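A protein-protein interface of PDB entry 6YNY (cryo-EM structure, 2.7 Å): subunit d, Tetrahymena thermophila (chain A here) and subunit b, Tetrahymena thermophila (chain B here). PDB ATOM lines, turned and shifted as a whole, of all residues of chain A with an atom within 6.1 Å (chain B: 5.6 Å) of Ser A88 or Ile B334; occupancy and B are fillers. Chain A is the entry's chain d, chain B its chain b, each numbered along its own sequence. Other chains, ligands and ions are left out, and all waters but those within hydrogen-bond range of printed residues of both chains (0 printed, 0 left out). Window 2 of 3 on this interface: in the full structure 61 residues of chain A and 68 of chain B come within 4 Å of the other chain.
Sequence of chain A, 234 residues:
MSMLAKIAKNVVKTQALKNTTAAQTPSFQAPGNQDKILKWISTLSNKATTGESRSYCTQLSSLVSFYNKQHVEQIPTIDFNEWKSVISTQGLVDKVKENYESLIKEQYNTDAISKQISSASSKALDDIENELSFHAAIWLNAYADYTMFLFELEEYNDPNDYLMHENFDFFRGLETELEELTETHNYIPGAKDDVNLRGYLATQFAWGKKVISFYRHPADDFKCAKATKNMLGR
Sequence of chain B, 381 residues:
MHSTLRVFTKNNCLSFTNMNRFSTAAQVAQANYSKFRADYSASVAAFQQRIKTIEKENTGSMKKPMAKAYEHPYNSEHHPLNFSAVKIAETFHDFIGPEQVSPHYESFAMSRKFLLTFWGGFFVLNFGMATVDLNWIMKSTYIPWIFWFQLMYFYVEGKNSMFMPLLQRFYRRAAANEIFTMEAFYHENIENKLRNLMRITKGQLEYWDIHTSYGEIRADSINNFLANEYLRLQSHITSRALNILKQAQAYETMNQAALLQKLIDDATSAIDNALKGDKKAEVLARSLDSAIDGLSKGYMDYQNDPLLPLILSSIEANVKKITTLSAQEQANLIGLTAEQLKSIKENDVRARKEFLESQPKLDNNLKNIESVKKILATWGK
OG of Ser A88 sits at hydrogen-bond distance from O of Trp A83 (2.7 Å).
OE2 of Glu B252 is in hydrogen-bond range of OG1 of Thr A89, 2.7 Å away.
Among the printed residues, merely in contact across the chains: Trp A83 with Leu B245 (3.3 Å), Ile A87 with Glu B252 (3.3 Å), Ser A88 with Glu B252 (3.5 Å), Ser A88 with Ile B334 (3.8 Å), Thr A89 with Ile B334 (3.3 Å), Thr A89 with Leu B336 (3.6 Å) and Gln A90 with Gln B330 (3.9 Å).
Printed residues of chain A that touch a printed residue of chain B: Trp A83, Ile A87, Ser A88, Thr A89 and Gln A90.
Hydrophobic or aromatic side chains of chain B within 4 Å of the printed part of chain A: Leu B245, Ile B334 and Leu B336.
Among the printed residues, 8 pairs touch across the chains.
Ser A88 touches two residues of chain B.
Of the printed residues of chain A, Ile B334 touches Ser A88 (3.8 Å) and Thr A89 (3.3 Å).
Of the printed residues of chain B, Ile A87 touches Glu B252 (3.3 Å).
Printed residues of chain B within 4 Å of Thr A89: Glu B252 (2.7 Å), Ile B334 (3.3 Å) and Leu B336 (3.6 Å).
Printed residues of chain B within 4 Å of Gln A90: Gln B330.
Glu B329 touches none of the printed residues of chain A.
Val A93 touches none of the printed residues of chain B.
The nearest residue of chain A that does not touch Ile B334 is Ile A87 (4.9 Å).
The nearest printed residue of chain B that does not touch Thr A89 is Gln B330 (5.7 Å).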
ATOM      1  N   PHE A  80     -14.591 -12.196  25.868  1.00  0.00           N
ATOM      2  CA  PHE A  80     -13.723 -12.824  24.877  1.00  0.00           C
ATOM      3  C   PHE A  80     -12.319 -12.238  24.911  1.00  0.00           C
ATOM      4  O   PHE A  80     -11.350 -12.927  24.570  1.00  0.00           O
ATOM      5  CB  PHE A  80     -14.329 -12.670  23.483  1.00  0.00           C
ATOM      6  CG  PHE A  80     -15.664 -13.338  23.328  1.00  0.00           C
ATOM      7  CD1 PHE A  80     -15.747 -14.669  22.953  1.00  0.00           C
ATOM      8  CD2 PHE A  80     -16.834 -12.637  23.562  1.00  0.00           C
ATOM      9  CE1 PHE A  80     -16.974 -15.285  22.812  1.00  0.00           C
ATOM     10  CE2 PHE A  80     -18.064 -13.249  23.423  1.00  0.00           C
ATOM     11  CZ  PHE A  80     -18.135 -14.575  23.047  1.00  0.00           C
ATOM     12  N   TRP A  83     -10.130 -14.251  27.437  1.00  0.00           N
ATOM     13  CA  TRP A  83      -9.696 -15.525  26.875  1.00  0.00           C
ATOM     14  C   TRP A  83      -8.750 -15.307  25.702  1.00  0.00           C
ATOM     15  O   TRP A  83      -7.788 -16.063  25.522  1.00  0.00           O
ATOM     16  CB  TRP A  83     -10.909 -16.347  26.442  1.00  0.00           C
ATOM     17  CG  TRP A  83     -11.913 -16.553  27.535  1.00  0.00           C
ATOM     18  CD1 TRP A  83     -13.075 -15.862  27.721  1.00  0.00           C
ATOM     19  CD2 TRP A  83     -11.844 -17.514  28.595  1.00  0.00           C
ATOM     20  NE1 TRP A  83     -13.734 -16.335  28.829  1.00  0.00           N
ATOM     21  CE2 TRP A  83     -12.999 -17.349  29.384  1.00  0.00           C
ATOM     22  CE3 TRP A  83     -10.918 -18.498  28.953  1.00  0.00           C
ATOM     23  CZ2 TRP A  83     -13.253 -18.131  30.509  1.00  0.00           C
ATOM     24  CZ3 TRP A  83     -11.171 -19.273  30.070  1.00  0.00           C
ATOM     25  CH2 TRP A  83     -12.329 -19.084  30.834  1.00  0.00           C
ATOM     26  N   LYS A  84      -9.013 -14.278  24.894  1.00  0.00           N
ATOM     27  CA  LYS A  84      -8.134 -13.968  23.773  1.00  0.00           C
ATOM     28  C   LYS A  84      -6.714 -13.682  24.240  1.00  0.00           C
ATOM     29  O   LYS A  84      -5.752 -13.975  23.521  1.00  0.00           O
ATOM     30  CB  LYS A  84      -8.693 -12.777  22.994  1.00  0.00           C
ATOM     31  CG  LYS A  84      -7.924 -12.425  21.728  1.00  0.00           C
ATOM     32  CD  LYS A  84      -8.266 -11.025  21.242  1.00  0.00           C
ATOM     33  CE  LYS A  84      -9.743 -10.891  20.899  1.00  0.00           C
ATOM     34  NZ  LYS A  84     -10.082  -9.525  20.418  1.00  0.00           N
ATOM     35  N   SER A  85      -6.560 -13.115  25.437  1.00  0.00           N
ATOM     36  CA  SER A  85      -5.251 -12.697  25.923  1.00  0.00           C
ATOM     37  C   SER A  85      -4.508 -13.843  26.601  1.00  0.00           C
ATOM     38  O   SER A  85      -3.355 -14.125  26.259  1.00  0.00           O
ATOM     39  CB  SER A  85      -5.404 -11.520  26.891  1.00  0.00           C
ATOM     40  OG  SER A  85      -6.218 -11.870  27.997  1.00  0.00           O
ATOM     41  N   VAL A  86      -5.150 -14.504  27.566  1.00  0.00           N
ATOM     42  CA  VAL A  86      -4.471 -15.545  28.337  1.00  0.00           C
ATOM     43  C   VAL A  86      -3.940 -16.629  27.403  1.00  0.00           C
ATOM     44  O   VAL A  86      -2.740 -16.925  27.383  1.00  0.00           O
ATOM     45  CB  VAL A  86      -5.406 -16.119  29.418  1.00  0.00           C
ATOM     46  CG1 VAL A  86      -6.687 -16.694  28.815  1.00  0.00           C
ATOM     47  CG2 VAL A  86      -4.678 -17.177  30.236  1.00  0.00           C
ATOM     48  N   ILE A  87      -4.827 -17.231  26.613  1.00  0.00           N
ATOM     49  CA  ILE A  87      -4.451 -18.314  25.710  1.00  0.00           C
ATOM     50  C   ILE A  87      -5.661 -18.677  24.860  1.00  0.00           C
ATOM     51  O   ILE A  87      -6.793 -18.719  25.356  1.00  0.00           O
ATOM     52  CB  ILE A  87      -3.927 -19.540  26.481  1.00  0.00           C
ATOM     53  CG1 ILE A  87      -3.458 -20.628  25.511  1.00  0.00           C
ATOM     54  CG2 ILE A  87      -5.004 -20.100  27.398  1.00  0.00           C
ATOM     55  CD1 ILE A  87      -2.255 -20.231  24.683  1.00  0.00           C
ATOM     56  N   SER A  88      -5.430 -18.941  23.577  1.00  0.00           N
ATOM     57  CA  SER A  88      -6.486 -19.367  22.668  1.00  0.00           C
ATOM     58  C   SER A  88      -5.852 -19.671  21.319  1.00  0.00           C
ATOM     59  O   SER A  88      -4.747 -19.211  21.016  1.00  0.00           O
ATOM     60  CB  SER A  88      -7.576 -18.302  22.515  1.00  0.00           C
ATOM     61  OG  SER A  88      -8.217 -18.039  23.752  1.00  0.00           O
ATOM     62  N   THR A  89      -6.567 -20.451  20.511  1.00  0.00           N
ATOM     63  CA  THR A  89      -6.112 -20.760  19.164  1.00  0.00           C
ATOM     64  C   THR A  89      -6.430 -19.596  18.235  1.00  0.00           C
ATOM     65  O   THR A  89      -7.537 -19.047  18.270  1.00  0.00           O
ATOM     66  CB  THR A  89      -6.773 -22.041  18.655  1.00  0.00           C
ATOM     67  OG1 THR A  89      -6.526 -23.110  19.577  1.00  0.00           O
ATOM     68  CG2 THR A  89      -6.222 -22.421  17.288  1.00  0.00           C
ATOM     69  N   GLN A  90      -5.456 -19.215  17.413  1.00  0.00           N
ATOM     70  CA  GLN A  90      -5.623 -18.079  16.517  1.00  0.00           C
ATOM     71  C   GLN A  90      -6.860 -18.255  15.647  1.00  0.00           C
ATOM     72  O   GLN A  90      -7.031 -19.283  14.986  1.00  0.00           O
ATOM     73  CB  GLN A  90      -4.373 -17.910  15.648  1.00  0.00           C
ATOM     74  CG  GLN A  90      -4.051 -19.100  14.750  1.00  0.00           C
ATOM     75  CD  GLN A  90      -4.720 -19.017  13.390  1.00  0.00           C
ATOM     76  OE1 GLN A  90      -5.456 -18.073  13.101  1.00  0.00           O
ATOM     77  NE2 GLN A  90      -4.465 -20.010  12.546  1.00  0.00           N
ATOM     78  N   LEU A  92      -9.893 -18.660  16.711  1.00  0.00           N
ATOM     79  CA  LEU A  92     -10.972 -19.365  17.394  1.00  0.00           C
ATOM     80  C   LEU A  92     -11.770 -18.421  18.286  1.00  0.00           C
ATOM     81  O   LEU A  92     -12.993 -18.308  18.154  1.00  0.00           O
ATOM     82  CB  LEU A  92     -10.397 -20.527  18.211  1.00  0.00           C
ATOM     83  CG  LEU A  92     -11.400 -21.516  18.814  1.00  0.00           C
ATOM     84  CD1 LEU A  92     -10.706 -22.829  19.140  1.00  0.00           C
ATOM     85  CD2 LEU A  92     -12.068 -20.948  20.059  1.00  0.00           C
ATOM     86  N   VAL A  93     -11.089 -17.731  19.206  1.00  0.00           N
ATOM     87  CA  VAL A  93     -11.787 -16.847  20.135  1.00  0.00           C
ATOM     88  C   VAL A  93     -12.579 -15.791  19.373  1.00  0.00           C
ATOM     89  O   VAL A  93     -13.678 -15.400  19.784  1.00  0.00           O
ATOM     90  CB  VAL A  93     -10.787 -16.209  21.117  1.00  0.00           C
ATOM     91  CG1 VAL A  93      -9.783 -15.339  20.374  1.00  0.00           C
ATOM     92  CG2 VAL A  93     -11.520 -15.397  22.174  1.00  0.00           C
ATOM     93  N   LEU B 245     -15.120 -23.158  24.838  1.00  0.00           N
ATOM     94  CA  LEU B 245     -13.878 -22.442  25.105  1.00  0.00           C
ATOM     95  C   LEU B 245     -13.072 -23.137  26.194  1.00  0.00           C
ATOM     96  O   LEU B 245     -11.869 -23.376  26.035  1.00  0.00           O
ATOM     97  CB  LEU B 245     -14.189 -20.998  25.500  1.00  0.00           C
ATOM     98  CG  LEU B 245     -13.070 -19.969  25.319  1.00  0.00           C
ATOM     99  CD1 LEU B 245     -13.625 -18.563  25.471  1.00  0.00           C
ATOM    100  CD2 LEU B 245     -11.939 -20.205  26.306  1.00  0.00           C
ATOM    101  N   GLU B 252      -5.708 -27.652  24.833  1.00  0.00           N
ATOM    102  CA  GLU B 252      -4.514 -26.836  24.635  1.00  0.00           C
ATOM    103  C   GLU B 252      -3.485 -27.096  25.728  1.00  0.00           C
ATOM    104  O   GLU B 252      -2.286 -27.214  25.448  1.00  0.00           O
ATOM    105  CB  GLU B 252      -4.894 -25.357  24.596  1.00  0.00           C
ATOM    106  CG  GLU B 252      -5.648 -24.947  23.341  1.00  0.00           C
ATOM    107  CD  GLU B 252      -5.963 -23.464  23.309  1.00  0.00           C
ATOM    108  OE1 GLU B 252      -5.637 -22.765  24.291  1.00  0.00           O
ATOM    109  OE2 GLU B 252      -6.534 -22.998  22.301  1.00  0.00           O
ATOM    110  N   THR B 253      -3.933 -27.189  26.981  1.00  0.00           N
ATOM    111  CA  THR B 253      -3.014 -27.498  28.071  1.00  0.00           C
ATOM    112  C   THR B 253      -2.447 -28.904  27.929  1.00  0.00           C
ATOM    113  O   THR B 253      -1.277 -29.144  28.245  1.00  0.00           O
ATOM    114  CB  THR B 253      -3.719 -27.339  29.418  1.00  0.00           C
ATOM    115  OG1 THR B 253      -4.887 -28.171  29.453  1.00  0.00           O
ATOM    116  CG2 THR B 253      -4.120 -25.888  29.646  1.00  0.00           C
ATOM    117  N   ASN B 255      -1.873 -30.547  25.111  1.00  0.00           N
ATOM    118  CA  ASN B 255      -0.848 -30.526  24.074  1.00  0.00           C
ATOM    119  C   ASN B 255       0.457 -29.945  24.605  1.00  0.00           C
ATOM    120  O   ASN B 255       1.543 -30.447  24.292  1.00  0.00           O
ATOM    121  CB  ASN B 255      -1.339 -29.725  22.867  1.00  0.00           C
ATOM    122  CG  ASN B 255      -2.496 -30.397  22.153  1.00  0.00           C
ATOM    123  OD1 ASN B 255      -3.661 -30.121  22.437  1.00  0.00           O
ATOM    124  ND2 ASN B 255      -2.179 -31.285  21.219  1.00  0.00           N
ATOM    125  N   GLU B 329       4.940 -20.511  17.260  1.00  0.00           N
ATOM    126  CA  GLU B 329       4.479 -21.030  18.542  1.00  0.00           C
ATOM    127  C   GLU B 329       2.959 -21.094  18.606  1.00  0.00           C
ATOM    128  O   GLU B 329       2.405 -21.896  19.366  1.00  0.00           O
ATOM    129  CB  GLU B 329       5.019 -20.163  19.679  1.00  0.00           C
ATOM    130  CG  GLU B 329       6.531 -20.208  19.822  1.00  0.00           C
ATOM    131  CD  GLU B 329       7.042 -19.287  20.912  1.00  0.00           C
ATOM    132  OE1 GLU B 329       6.215 -18.590  21.538  1.00  0.00           O
ATOM    133  OE2 GLU B 329       8.269 -19.259  21.142  1.00  0.00           O
ATOM    134  N   GLN B 330       2.270 -20.260  17.823  1.00  0.00           N
ATOM    135  CA  GLN B 330       0.811 -20.275  17.822  1.00  0.00           C
ATOM    136  C   GLN B 330       0.279 -21.675  17.539  1.00  0.00           C
ATOM    137  O   GLN B 330      -0.638 -22.155  18.216  1.00  0.00           O
ATOM    138  CB  GLN B 330       0.281 -19.281  16.787  1.00  0.00           C
ATOM    139  CG  GLN B 330       0.687 -17.841  17.047  1.00  0.00           C
ATOM    140  CD  GLN B 330       0.134 -16.883  16.012  1.00  0.00           C
ATOM    141  OE1 GLN B 330      -0.601 -17.282  15.108  1.00  0.00           O
ATOM    142  NE2 GLN B 330       0.489 -15.609  16.135  1.00  0.00           N
ATOM    143  N   ALA B 331       0.849 -22.347  16.539  1.00  0.00           N
ATOM    144  CA  ALA B 331       0.425 -23.694  16.184  1.00  0.00           C
ATOM    145  C   ALA B 331       1.271 -24.766  16.853  1.00  0.00           C
ATOM    146  O   ALA B 331       0.748 -25.831  17.202  1.00  0.00           O
ATOM    147  CB  ALA B 331       0.481 -23.880  14.665  1.00  0.00           C
ATOM    148  N   ASN B 332       2.567 -24.509  17.041  1.00  0.00           N
ATOM    149  CA  ASN B 332       3.437 -25.498  17.666  1.00  0.00           C
ATOM    150  C   ASN B 332       3.018 -25.765  19.106  1.00  0.00           C
ATOM    151  O   ASN B 332       2.937 -26.920  19.539  1.00  0.00           O
ATOM    152  CB  ASN B 332       4.890 -25.024  17.607  1.00  0.00           C
ATOM    153  CG  ASN B 332       5.841 -25.972  18.308  1.00  0.00           C
ATOM    154  OD1 ASN B 332       6.131 -25.817  19.494  1.00  0.00           O
ATOM    155  ND2 ASN B 332       6.334 -26.963  17.574  1.00  0.00           N
ATOM    156  N   LEU B 333       2.747 -24.702  19.867  1.00  0.00           N
ATOM    157  CA  LEU B 333       2.340 -24.873  21.259  1.00  0.00           C
ATOM    158  C   LEU B 333       1.049 -25.675  21.357  1.00  0.00           C
ATOM    159  O   LEU B 333       0.943 -26.608  22.161  1.00  0.00           O
ATOM    160  CB  LEU B 333       2.177 -23.507  21.926  1.00  0.00           C
ATOM    161  CG  LEU B 333       1.563 -23.510  23.329  1.00  0.00           C
ATOM    162  CD1 LEU B 333       2.286 -24.490  24.242  1.00  0.00           C
ATOM    163  CD2 LEU B 333       1.578 -22.108  23.920  1.00  0.00           C
ATOM    164  N   ILE B 334       0.057 -25.326  20.548  1.00  0.00           N
ATOM    165  CA  ILE B 334      -1.254 -25.971  20.576  1.00  0.00           C
ATOM    166  C   ILE B 334      -1.495 -26.539  19.182  1.00  0.00           C
ATOM    167  O   ILE B 334      -2.002 -25.860  18.285  1.00  0.00           O
ATOM    168  CB  ILE B 334      -2.369 -25.011  20.999  1.00  0.00           C
ATOM    169  CG1 ILE B 334      -2.223 -23.661  20.287  1.00  0.00           C
ATOM    170  CG2 ILE B 334      -2.344 -24.817  22.506  1.00  0.00           C
ATOM    171  CD1 ILE B 334      -3.359 -22.696  20.560  1.00  0.00           C
ATOM    172  N   GLY B 335      -1.131 -27.805  18.992  1.00  0.00           N
ATOM    173  CA  GLY B 335      -1.336 -28.471  17.721  1.00  0.00           C
ATOM    174  C   GLY B 335      -2.658 -29.207  17.651  1.00  0.00           C
ATOM    175  O   GLY B 335      -2.685 -30.441  17.648  1.00  0.00           O
ATOM    176  N   LEU B 336      -3.762 -28.463  17.596  1.00  0.00           N
ATOM    177  CA  LEU B 336      -5.082 -29.080  17.541  1.00  0.00           C
ATOM    178  C   LEU B 336      -5.232 -29.903  16.268  1.00  0.00           C
ATOM    179  O   LEU B 336      -5.293 -29.349  15.165  1.00  0.00           O
ATOM    180  CB  LEU B 336      -6.180 -28.017  17.617  1.00  0.00           C
ATOM    181  CG  LEU B 336      -6.389 -27.357  18.983  1.00  0.00           C
ATOM    182  CD1 LEU B 336      -5.234 -26.433  19.327  1.00  0.00           C
ATOM    183  CD2 LEU B 336      -7.708 -26.601  19.014  1.00  0.00           C
